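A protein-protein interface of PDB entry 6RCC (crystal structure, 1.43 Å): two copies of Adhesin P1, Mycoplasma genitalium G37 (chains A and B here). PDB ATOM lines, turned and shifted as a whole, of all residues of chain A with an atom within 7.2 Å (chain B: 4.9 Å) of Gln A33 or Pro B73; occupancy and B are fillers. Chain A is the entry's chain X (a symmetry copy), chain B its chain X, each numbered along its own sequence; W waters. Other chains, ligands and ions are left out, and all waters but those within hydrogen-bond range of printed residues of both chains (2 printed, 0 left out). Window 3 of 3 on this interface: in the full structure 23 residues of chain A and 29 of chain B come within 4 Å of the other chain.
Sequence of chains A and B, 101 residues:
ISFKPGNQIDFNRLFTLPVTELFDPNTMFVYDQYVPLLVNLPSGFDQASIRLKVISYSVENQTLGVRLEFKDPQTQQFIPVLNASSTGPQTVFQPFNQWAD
The side-chain amide nitrogen (NE2) of Gln A33 lies within hydrogen-bond range of the backbone carbonyl oxygen (O) of Lys B71 (2.8 Å).
The backbone NH (N) of Lys B71 lies within hydrogen-bond range of the backbone carbonyl oxygen (O) of Ser B49 (2.8 Å). The side-chain carboxylate of Asp B72 lies close to the backbone NH of Gln B74, 3.2 Å away. The backbone carbonyl oxygen (O) of Pro B73 lies within hydrogen-bond range of the side-chain amide nitrogen (NE2) of Gln B76 (2.9 Å). The backbone carbonyl oxygen (O) of Leu A22 is in hydrogen-bond range of the backbone NH (N) of Tyr A31 (3.0 Å). NE2 of Gln A33 sits at hydrogen-bond distance from OH of Tyr A34 (3.3 Å).
Among the printed residues, merely in contact across the chains: Phe A15 with Phe B70 (3.6 Å), Leu A17 with Phe B70 (3.6 Å), Tyr A31 with Pro B73 (3.5 Å), Tyr A31 with Gln B74 (3.4 Å), Gln A33 with Phe B45 (3.4 Å), Gln A33 with Ser B49 (3.8 Å), Gln A33 with Pro B73 (3.8 Å), Tyr A34 with Phe B70 (3.5 Å), Tyr A34 with Pro B73 (3.8 Å) and Pro A36 with Phe B45 (3.8 Å).
Of the printed residues of chain B, Phe A15 touches Phe B70. Of chain B, only Phe B45 (3.4 Å), Ser B49 (3.8 Å), Lys B71 (2.8 Å) and Pro B73 (3.8 Å) come within 4 Å of Gln A33. Of the printed residues of chain B, Tyr A34 touches Phe B70 and Pro B73. Val A35 touches none of the printed residues of chain B. Printed residues of chain A within 4 Å of Ser B49: Gln A33. Printed residues of chain A within 4 Å of Gln B74: Tyr A31 (3.4 Å). The nearest residue of chain B that does not touch Gln A33 is Phe B70 (4.6 Å). The nearest printed residue of chain A that does not touch Pro B73 is Glu A21 (4.8 Å).
Of the 9 printed residues of chain B, 6 touch a printed residue of chain A. Hydrophobic or aromatic side chains of chain B that line the printed part of chain A: Phe B45, Phe B70 and Pro B73. Of the 16 printed residues of chain A, 6 touch a printed residue of chain B. Hydrophobic or aromatic side chains of chain A within 4 Å of the printed part of chain B: Phe A15, Leu A17, Tyr A31, Tyr A34 and Pro A36. Among the printed residues, 11 pairs touch across the chains. Among the printed residues, no Asp or Glu carboxylate lies within 4 Å of a Lys or Arg side-chain nitrogen of the other chain.
No position is printed for both chains.
Water W1 lies within hydrogen-bond range of OE2 of Glu A21, NE2 of Gln B74 and OD2 of Asp B72. Water W2 lies within hydrogen-bond range of OD2 of Asp B72 (2.8 Å) and OE2 of Glu A21 (2.8 Å).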
ATOM      1  N   PHE A  15       4.118 -23.301 -31.415  1.00  0.00           N
ATOM      2  CA  PHE A  15       4.482 -24.020 -30.218  1.00  0.00           C
ATOM      3  C   PHE A  15       3.805 -23.487 -28.987  1.00  0.00           C
ATOM      4  O   PHE A  15       3.801 -22.284 -28.753  1.00  0.00           O
ATOM      5  CB  PHE A  15       6.019 -23.935 -30.035  1.00  0.00           C
ATOM      6  CG  PHE A  15       6.537 -24.772 -28.886  1.00  0.00           C
ATOM      7  CD1 PHE A  15       6.735 -26.143 -29.036  1.00  0.00           C
ATOM      8  CD2 PHE A  15       6.748 -24.205 -27.635  1.00  0.00           C
ATOM      9  CE1 PHE A  15       7.161 -26.929 -27.948  1.00  0.00           C
ATOM     10  CE2 PHE A  15       7.192 -24.987 -26.562  1.00  0.00           C
ATOM     11  CZ  PHE A  15       7.379 -26.338 -26.721  1.00  0.00           C
ATOM     12  N   LEU A  17       2.895 -25.268 -24.728  1.00  0.00           N
ATOM     13  CA  LEU A  17       3.098 -26.411 -23.877  1.00  0.00           C
ATOM     14  C   LEU A  17       2.433 -26.147 -22.546  1.00  0.00           C
ATOM     15  O   LEU A  17       2.497 -25.019 -22.057  1.00  0.00           O
ATOM     16  CB  LEU A  17       4.617 -26.487 -23.626  1.00  0.00           C
ATOM     17  CG  LEU A  17       5.285 -27.757 -23.288  1.00  0.00           C
ATOM     18  CD1 LEU A  17       5.172 -28.777 -24.412  1.00  0.00           C
ATOM     19  CD2 LEU A  17       6.756 -27.492 -23.032  1.00  0.00           C
ATOM     20  N   GLU A  21       5.119 -29.314 -18.381  1.00  0.00           N
ATOM     21  CA  GLU A  21       6.065 -29.940 -19.304  1.00  0.00           C
ATOM     22  C   GLU A  21       7.361 -29.116 -19.436  1.00  0.00           C
ATOM     23  O   GLU A  21       8.303 -29.556 -20.106  1.00  0.00           O
ATOM     24  CB  GLU A  21       5.415 -30.124 -20.697  1.00  0.00           C
ATOM     25  CG  GLU A  21       4.185 -31.029 -20.705  1.00  0.00           C
ATOM     26  CD  GLU A  21       4.425 -32.464 -20.278  1.00  0.00           C
ATOM     27  OE1 GLU A  21       3.544 -33.040 -19.600  1.00  0.00           O
ATOM     28  OE2 GLU A  21       5.505 -33.005 -20.604  1.00  0.00           O
ATOM     29  N   LEU A  22       7.411 -27.920 -18.812  1.00  0.00           N
ATOM     30  CA  LEU A  22       8.550 -27.017 -18.974  1.00  0.00           C
ATOM     31  C   LEU A  22       9.722 -27.325 -18.111  1.00  0.00           C
ATOM     32  O   LEU A  22      10.811 -26.795 -18.382  1.00  0.00           O
ATOM     33  CB  LEU A  22       8.120 -25.582 -18.708  1.00  0.00           C
ATOM     34  CG  LEU A  22       7.245 -24.950 -19.799  1.00  0.00           C
ATOM     35  CD1 LEU A  22       6.636 -23.615 -19.327  1.00  0.00           C
ATOM     36  CD2 LEU A  22       8.049 -24.743 -21.070  1.00  0.00           C
ATOM     37  N   PHE A  23       9.535 -28.122 -17.052  1.00  0.00           N
ATOM     38  CA  PHE A  23      10.604 -28.348 -16.104  1.00  0.00           C
ATOM     39  C   PHE A  23      10.712 -29.775 -15.677  1.00  0.00           C
ATOM     40  O   PHE A  23       9.731 -30.525 -15.744  1.00  0.00           O
ATOM     41  CB  PHE A  23      10.400 -27.454 -14.835  1.00  0.00           C
ATOM     42  CG  PHE A  23       9.056 -27.652 -14.159  1.00  0.00           C
ATOM     43  CD1 PHE A  23       8.894 -28.607 -13.154  1.00  0.00           C
ATOM     44  CD2 PHE A  23       7.960 -26.882 -14.519  1.00  0.00           C
ATOM     45  CE1 PHE A  23       7.634 -28.817 -12.555  1.00  0.00           C
ATOM     46  CE2 PHE A  23       6.708 -27.086 -13.915  1.00  0.00           C
ATOM     47  CZ  PHE A  23       6.551 -28.053 -12.939  1.00  0.00           C
ATOM     48  N   ASP A  24      11.908 -30.145 -15.199  1.00  0.00           N
ATOM     49  CA  ASP A  24      12.142 -31.472 -14.670  1.00  0.00           C
ATOM     50  C   ASP A  24      11.389 -31.559 -13.343  1.00  0.00           C
ATOM     51  O   ASP A  24      11.642 -30.761 -12.447  1.00  0.00           O
ATOM     52  CB  ASP A  24      13.634 -31.685 -14.469  1.00  0.00           C
ATOM     53  CG  ASP A  24      13.985 -33.075 -13.982  1.00  0.00           C
ATOM     54  OD1 ASP A  24      13.364 -33.537 -12.978  1.00  0.00           O
ATOM     55  OD2 ASP A  24      14.892 -33.688 -14.571  1.00  0.00           O
ATOM     56  N   VAL A  30      13.901 -25.644 -15.019  1.00  0.00           N
ATOM     57  CA  VAL A  30      13.364 -25.615 -16.389  1.00  0.00           C
ATOM     58  C   VAL A  30      14.331 -26.412 -17.279  1.00  0.00           C
ATOM     59  O   VAL A  30      15.555 -26.286 -17.131  1.00  0.00           O
ATOM     60  CB  VAL A  30      13.244 -24.150 -16.869  1.00  0.00           C
ATOM     61  CG1 VAL A  30      12.908 -24.052 -18.371  1.00  0.00           C
ATOM     62  CG2 VAL A  30      12.220 -23.394 -16.027  1.00  0.00           C
ATOM     63  N   TYR A  31      13.785 -27.213 -18.218  1.00  0.00           N
ATOM     64  CA  TYR A  31      14.640 -27.960 -19.135  1.00  0.00           C
ATOM     65  C   TYR A  31      15.465 -26.944 -19.958  1.00  0.00           C
ATOM     66  O   TYR A  31      14.966 -25.884 -20.355  1.00  0.00           O
ATOM     67  CB  TYR A  31      13.801 -28.812 -20.081  1.00  0.00           C
ATOM     68  CG  TYR A  31      13.098 -29.936 -19.384  1.00  0.00           C
ATOM     69  CD1 TYR A  31      13.812 -31.004 -18.854  1.00  0.00           C
ATOM     70  CD2 TYR A  31      11.708 -30.009 -19.371  1.00  0.00           C
ATOM     71  CE1 TYR A  31      13.161 -32.078 -18.258  1.00  0.00           C
ATOM     72  CE2 TYR A  31      11.046 -31.089 -18.803  1.00  0.00           C
ATOM     73  CZ  TYR A  31      11.775 -32.115 -18.239  1.00  0.00           C
ATOM     74  OH  TYR A  31      11.138 -33.192 -17.664  1.00  0.00           O
ATOM     75  N   ASP A  32      16.717 -27.262 -20.207  1.00  0.00           N
ATOM     76  CA  ASP A  32      17.621 -26.385 -20.932  1.00  0.00           C
ATOM     77  C   ASP A  32      17.017 -25.856 -22.238  1.00  0.00           C
ATOM     78  O   ASP A  32      17.168 -24.665 -22.524  1.00  0.00           O
ATOM     79  CB  ASP A  32      18.919 -27.122 -21.298  1.00  0.00           C
ATOM     80  CG  ASP A  32      19.780 -27.561 -20.137  1.00  0.00           C
ATOM     81  OD1 ASP A  32      19.569 -27.056 -19.017  1.00  0.00           O
ATOM     82  OD2 ASP A  32      20.683 -28.399 -20.354  1.00  0.00           O
ATOM     83  N   GLN A  33      16.304 -26.729 -22.991  1.00  0.00           N
ATOM     84  CA  GLN A  33      15.779 -26.355 -24.296  1.00  0.00           C
ATOM     85  C   GLN A  33      14.734 -25.263 -24.219  1.00  0.00           C
ATOM     86  O   GLN A  33      14.537 -24.572 -25.208  1.00  0.00           O
ATOM     87  CB  GLN A  33      15.263 -27.578 -25.086  1.00  0.00           C
ATOM     88  CG  GLN A  33      13.982 -28.220 -24.548  1.00  0.00           C
ATOM     89  CD  GLN A  33      13.718 -29.604 -25.143  1.00  0.00           C
ATOM     90  OE1 GLN A  33      14.508 -30.537 -24.981  1.00  0.00           O
ATOM     91  NE2 GLN A  33      12.574 -29.792 -25.813  1.00  0.00           N
ATOM     92  N   TYR A  34      14.105 -25.073 -23.035  1.00  0.00           N
ATOM     93  CA  TYR A  34      13.062 -24.058 -22.906  1.00  0.00           C
ATOM     94  C   TYR A  34      13.518 -22.765 -22.278  1.00  0.00           C
ATOM     95  O   TYR A  34      12.753 -21.812 -22.302  1.00  0.00           O
ATOM     96  CB  TYR A  34      11.839 -24.607 -22.151  1.00  0.00           C
ATOM     97  CG  TYR A  34      11.234 -25.838 -22.780  1.00  0.00           C
ATOM     98  CD1 TYR A  34      11.005 -25.902 -24.161  1.00  0.00           C
ATOM     99  CD2 TYR A  34      10.894 -26.944 -22.007  1.00  0.00           C
ATOM    100  CE1 TYR A  34      10.473 -27.049 -24.749  1.00  0.00           C
ATOM    101  CE2 TYR A  34      10.342 -28.088 -22.581  1.00  0.00           C
ATOM    102  CZ  TYR A  34      10.132 -28.131 -23.956  1.00  0.00           C
ATOM    103  OH  TYR A  34       9.610 -29.273 -24.519  1.00  0.00           O
ATOM    104  N   VAL A  35      14.757 -22.692 -21.749  1.00  0.00           N
ATOM    105  CA  VAL A  35      15.231 -21.452 -21.112  1.00  0.00           C
ATOM    106  C   VAL A  35      15.158 -20.272 -22.108  1.00  0.00           C
ATOM    107  O   VAL A  35      14.581 -19.251 -21.755  1.00  0.00           O
ATOM    108  CB  VAL A  35      16.607 -21.615 -20.437  1.00  0.00           C
ATOM    109  CG1 VAL A  35      17.172 -20.268 -19.942  1.00  0.00           C
ATOM    110  CG2 VAL A  35      16.540 -22.648 -19.315  1.00  0.00           C
ATOM    111  N   PRO A  36      15.604 -20.400 -23.386  1.00  0.00           N
ATOM    112  CA  PRO A  36      15.496 -19.264 -24.321  1.00  0.00           C
ATOM    113  C   PRO A  36      14.090 -18.907 -24.722  1.00  0.00           C
ATOM    114  O   PRO A  36      13.850 -17.816 -25.239  1.00  0.00           O
ATOM    115  CB  PRO A  36      16.282 -19.719 -25.558  1.00  0.00           C
ATOM    116  CG  PRO A  36      17.021 -20.896 -25.153  1.00  0.00           C
ATOM    117  CD  PRO A  36      16.322 -21.527 -24.015  1.00  0.00           C
ATOM    118  N   LEU A  37      13.162 -19.818 -24.493  1.00  0.00           N
ATOM    119  CA  LEU A  37      11.788 -19.566 -24.827  1.00  0.00           C
ATOM    120  C   LEU A  37      11.133 -18.716 -23.733  1.00  0.00           C
ATOM    121  O   LEU A  37      10.313 -17.867 -24.044  1.00  0.00           O
ATOM    122  CB  LEU A  37      11.103 -20.931 -24.966  1.00  0.00           C
ATOM    123  CG  LEU A  37       9.680 -20.954 -25.399  1.00  0.00           C
ATOM    124  CD1 LEU A  37       9.502 -20.261 -26.757  1.00  0.00           C
ATOM    125  CD2 LEU A  37       9.219 -22.385 -25.482  1.00  0.00           C
ATOM    126  N   LEU A  38      11.507 -18.928 -22.465  1.00  0.00           N
ATOM    127  CA  LEU A  38      10.968 -18.208 -21.312  1.00  0.00           C
ATOM    128  C   LEU A  38      11.609 -16.879 -21.046  1.00  0.00           C
ATOM    129  O   LEU A  38      10.969 -15.981 -20.477  1.00  0.00           O
ATOM    130  CB  LEU A  38      11.061 -19.077 -20.044  1.00  0.00           C
ATOM    131  CG  LEU A  38      10.415 -20.460 -20.177  1.00  0.00           C
ATOM    132  CD1 LEU A  38      10.533 -21.245 -18.879  1.00  0.00           C
ATOM    133  CD2 LEU A  38       8.970 -20.373 -20.617  1.00  0.00           C
ATOM    134  N   GLN A  47      23.975 -19.989 -22.775  1.00  0.00           N
ATOM    135  CA  GLN A  47      22.946 -20.515 -21.871  1.00  0.00           C
ATOM    136  C   GLN A  47      23.437 -21.517 -20.866  1.00  0.00           C
ATOM    137  O   GLN A  47      22.726 -21.754 -19.888  1.00  0.00           O
ATOM    138  CB  GLN A  47      21.837 -21.157 -22.640  1.00  0.00           C
ATOM    139  CG  GLN A  47      21.042 -20.201 -23.452  1.00  0.00           C
ATOM    140  CD  GLN A  47      20.577 -20.955 -24.640  1.00  0.00           C
ATOM    141  OE1 GLN A  47      19.934 -22.004 -24.517  1.00  0.00           O
ATOM    142  NE2 GLN A  47      20.946 -20.465 -25.804  1.00  0.00           N
ATOM    143  N   PHE B  45      17.714 -20.197 -29.076  1.00  0.00           N
ATOM    144  CA  PHE B  45      16.943 -21.450 -29.091  1.00  0.00           C
ATOM    145  C   PHE B  45      17.707 -22.624 -29.773  1.00  0.00           C
ATOM    146  O   PHE B  45      18.307 -22.420 -30.821  1.00  0.00           O
ATOM    147  CB  PHE B  45      15.568 -21.207 -29.696  1.00  0.00           C
ATOM    148  CG  PHE B  45      14.653 -22.396 -29.568  1.00  0.00           C
ATOM    149  CD1 PHE B  45      14.009 -22.665 -28.369  1.00  0.00           C
ATOM    150  CD2 PHE B  45      14.506 -23.294 -30.618  1.00  0.00           C
ATOM    151  CE1 PHE B  45      13.207 -23.802 -28.233  1.00  0.00           C
ATOM    152  CE2 PHE B  45      13.667 -24.401 -30.492  1.00  0.00           C
ATOM    153  CZ  PHE B  45      13.026 -24.644 -29.302  1.00  0.00           C
ATOM    154  N   SER B  49      16.032 -29.321 -30.869  1.00  0.00           N
ATOM    155  CA  SER B  49      14.861 -29.738 -30.122  1.00  0.00           C
ATOM    156  C   SER B  49      13.581 -29.652 -30.942  1.00  0.00           C
ATOM    157  O   SER B  49      12.540 -30.008 -30.410  1.00  0.00           O
ATOM    158  CB  SER B  49      14.736 -28.952 -28.821  1.00  0.00           C
ATOM    159  OG  SER B  49      14.389 -27.608 -29.096  1.00  0.00           O
ATOM    160  N   PHE B  70       8.423 -31.404 -31.616  1.00  0.00           N
ATOM    161  CA  PHE B  70       9.492 -31.026 -30.703  1.00  0.00           C
ATOM    162  C   PHE B  70       9.953 -32.249 -29.938  1.00  0.00           C
ATOM    163  O   PHE B  70       9.199 -33.210 -29.784  1.00  0.00           O
ATOM    164  CB  PHE B  70       9.031 -29.907 -29.750  1.00  0.00           C
ATOM    165  CG  PHE B  70       7.997 -30.351 -28.743  1.00  0.00           C
ATOM    166  CD1 PHE B  70       6.656 -30.471 -29.103  1.00  0.00           C
ATOM    167  CD2 PHE B  70       8.359 -30.655 -27.438  1.00  0.00           C
ATOM    168  CE1 PHE B  70       5.705 -30.905 -28.180  1.00  0.00           C
ATOM    169  CE2 PHE B  70       7.415 -31.110 -26.525  1.00  0.00           C
ATOM    170  CZ  PHE B  70       6.087 -31.216 -26.894  1.00  0.00           C
ATOM    171  N   LYS B  71      11.174 -32.198 -29.460  1.00  0.00           N
ATOM    172  CA  LYS B  71      11.743 -33.307 -28.716  1.00  0.00           C
ATOM    173  C   LYS B  71      11.300 -33.290 -27.263  1.00  0.00           C
ATOM    174  O   LYS B  71      11.586 -32.316 -26.573  1.00  0.00           O
ATOM    175  CB  LYS B  71      13.276 -33.247 -28.815  1.00  0.00           C
ATOM    176  CG  LYS B  71      14.028 -34.452 -28.243  1.00  0.00           C
ATOM    177  CD  LYS B  71      15.196 -34.859 -29.151  1.00  0.00           C
ATOM    178  CE  LYS B  71      16.356 -33.883 -29.151  1.00  0.00           C
ATOM    179  NZ  LYS B  71      17.322 -34.173 -30.243  1.00  0.00           N
ATOM    180  N   ASP B  72      10.619 -34.350 -26.805  1.00  0.00           N
ATOM    181  CA  ASP B  72      10.212 -34.481 -25.408  1.00  0.00           C
ATOM    182  C   ASP B  72      11.514 -34.599 -24.578  1.00  0.00           C
ATOM    183  O   ASP B  72      12.343 -35.456 -24.875  1.00  0.00           O
ATOM    184  CB  ASP B  72       9.306 -35.704 -25.217  1.00  0.00           C
ATOM    185  CG  ASP B  72       8.817 -35.854 -23.789  1.00  0.00           C
ATOM    186  OD1 ASP B  72       9.469 -36.578 -23.015  1.00  0.00           O
ATOM    187  OD2 ASP B  72       7.790 -35.239 -23.449  1.00  0.00           O
ATOM    188  N   PRO B  73      11.753 -33.698 -23.602  1.00  0.00           N
ATOM    189  CA  PRO B  73      13.027 -33.720 -22.862  1.00  0.00           C
ATOM    190  C   PRO B  73      13.353 -35.009 -22.119  1.00  0.00           C
ATOM    191  O   PRO B  73      14.535 -35.285 -21.899  1.00  0.00           O
ATOM    192  CB  PRO B  73      12.876 -32.559 -21.880  1.00  0.00           C
ATOM    193  CG  PRO B  73      11.887 -31.656 -22.512  1.00  0.00           C
ATOM    194  CD  PRO B  73      10.902 -32.581 -23.147  1.00  0.00           C
ATOM    195  N   GLN B  74      12.324 -35.791 -21.746  1.00  0.00           N
ATOM    196  CA  GLN B  74      12.468 -37.044 -21.001  1.00  0.00           C
ATOM    197  C   GLN B  74      12.787 -38.222 -21.918  1.00  0.00           C
ATOM    198  O   GLN B  74      13.841 -38.850 -21.766  1.00  0.00           O
ATOM    199  CB  GLN B  74      11.198 -37.343 -20.169  1.00  0.00           C
ATOM    200  CG  GLN B  74      10.767 -36.207 -19.226  1.00  0.00           C
ATOM    201  CD  GLN B  74       9.555 -36.544 -18.384  1.00  0.00           C
ATOM    202  OE1 GLN B  74       9.547 -37.506 -17.608  1.00  0.00           O
ATOM    203  NE2 GLN B  74       8.511 -35.737 -18.495  1.00  0.00           N
ATOM    204  N   THR B  75      11.876 -38.531 -22.855  1.00  0.00           N
ATOM    205  CA  THR B  75      12.005 -39.670 -23.769  1.00  0.00           C
ATOM    206  C   THR B  75      12.951 -39.426 -24.943  1.00  0.00           C
ATOM    207  O   THR B  75      13.499 -40.384 -25.487  1.00  0.00           O
ATOM    208  CB  THR B  75      10.625 -40.124 -24.256  1.00  0.00           C
ATOM    209  OG1 THR B  75      10.037 -39.078 -25.034  1.00  0.00           O
ATOM    210  CG2 THR B  75       9.697 -40.514 -23.111  1.00  0.00           C
ATOM    211  N   GLN B  76      13.104 -38.162 -25.367  1.00  0.00           N
ATOM    212  CA  GLN B  76      13.920 -37.756 -26.525  1.00  0.00           C
ATOM    213  C   GLN B  76      13.267 -38.172 -27.846  1.00  0.00           C
ATOM    214  O   GLN B  76      13.944 -38.271 -28.877  1.00  0.00           O
ATOM    215  CB  GLN B  76      15.395 -38.219 -26.422  1.00  0.00           C
ATOM    216  CG  GLN B  76      16.143 -37.685 -25.197  1.00  0.00           C
ATOM    217  CD  GLN B  76      16.485 -36.224 -25.312  1.00  0.00           C
ATOM    218  OE1 GLN B  76      17.158 -35.782 -26.252  1.00  0.00           O
ATOM    219  NE2 GLN B  76      16.030 -35.439 -24.347  1.00  0.00           N
HETATM  220  O   HOH W   1       6.663 -35.455 -20.576  1.00  0.00           O
HETATM  221  O   HOH W   2       6.535 -32.786 -23.246  1.00  0.00           O
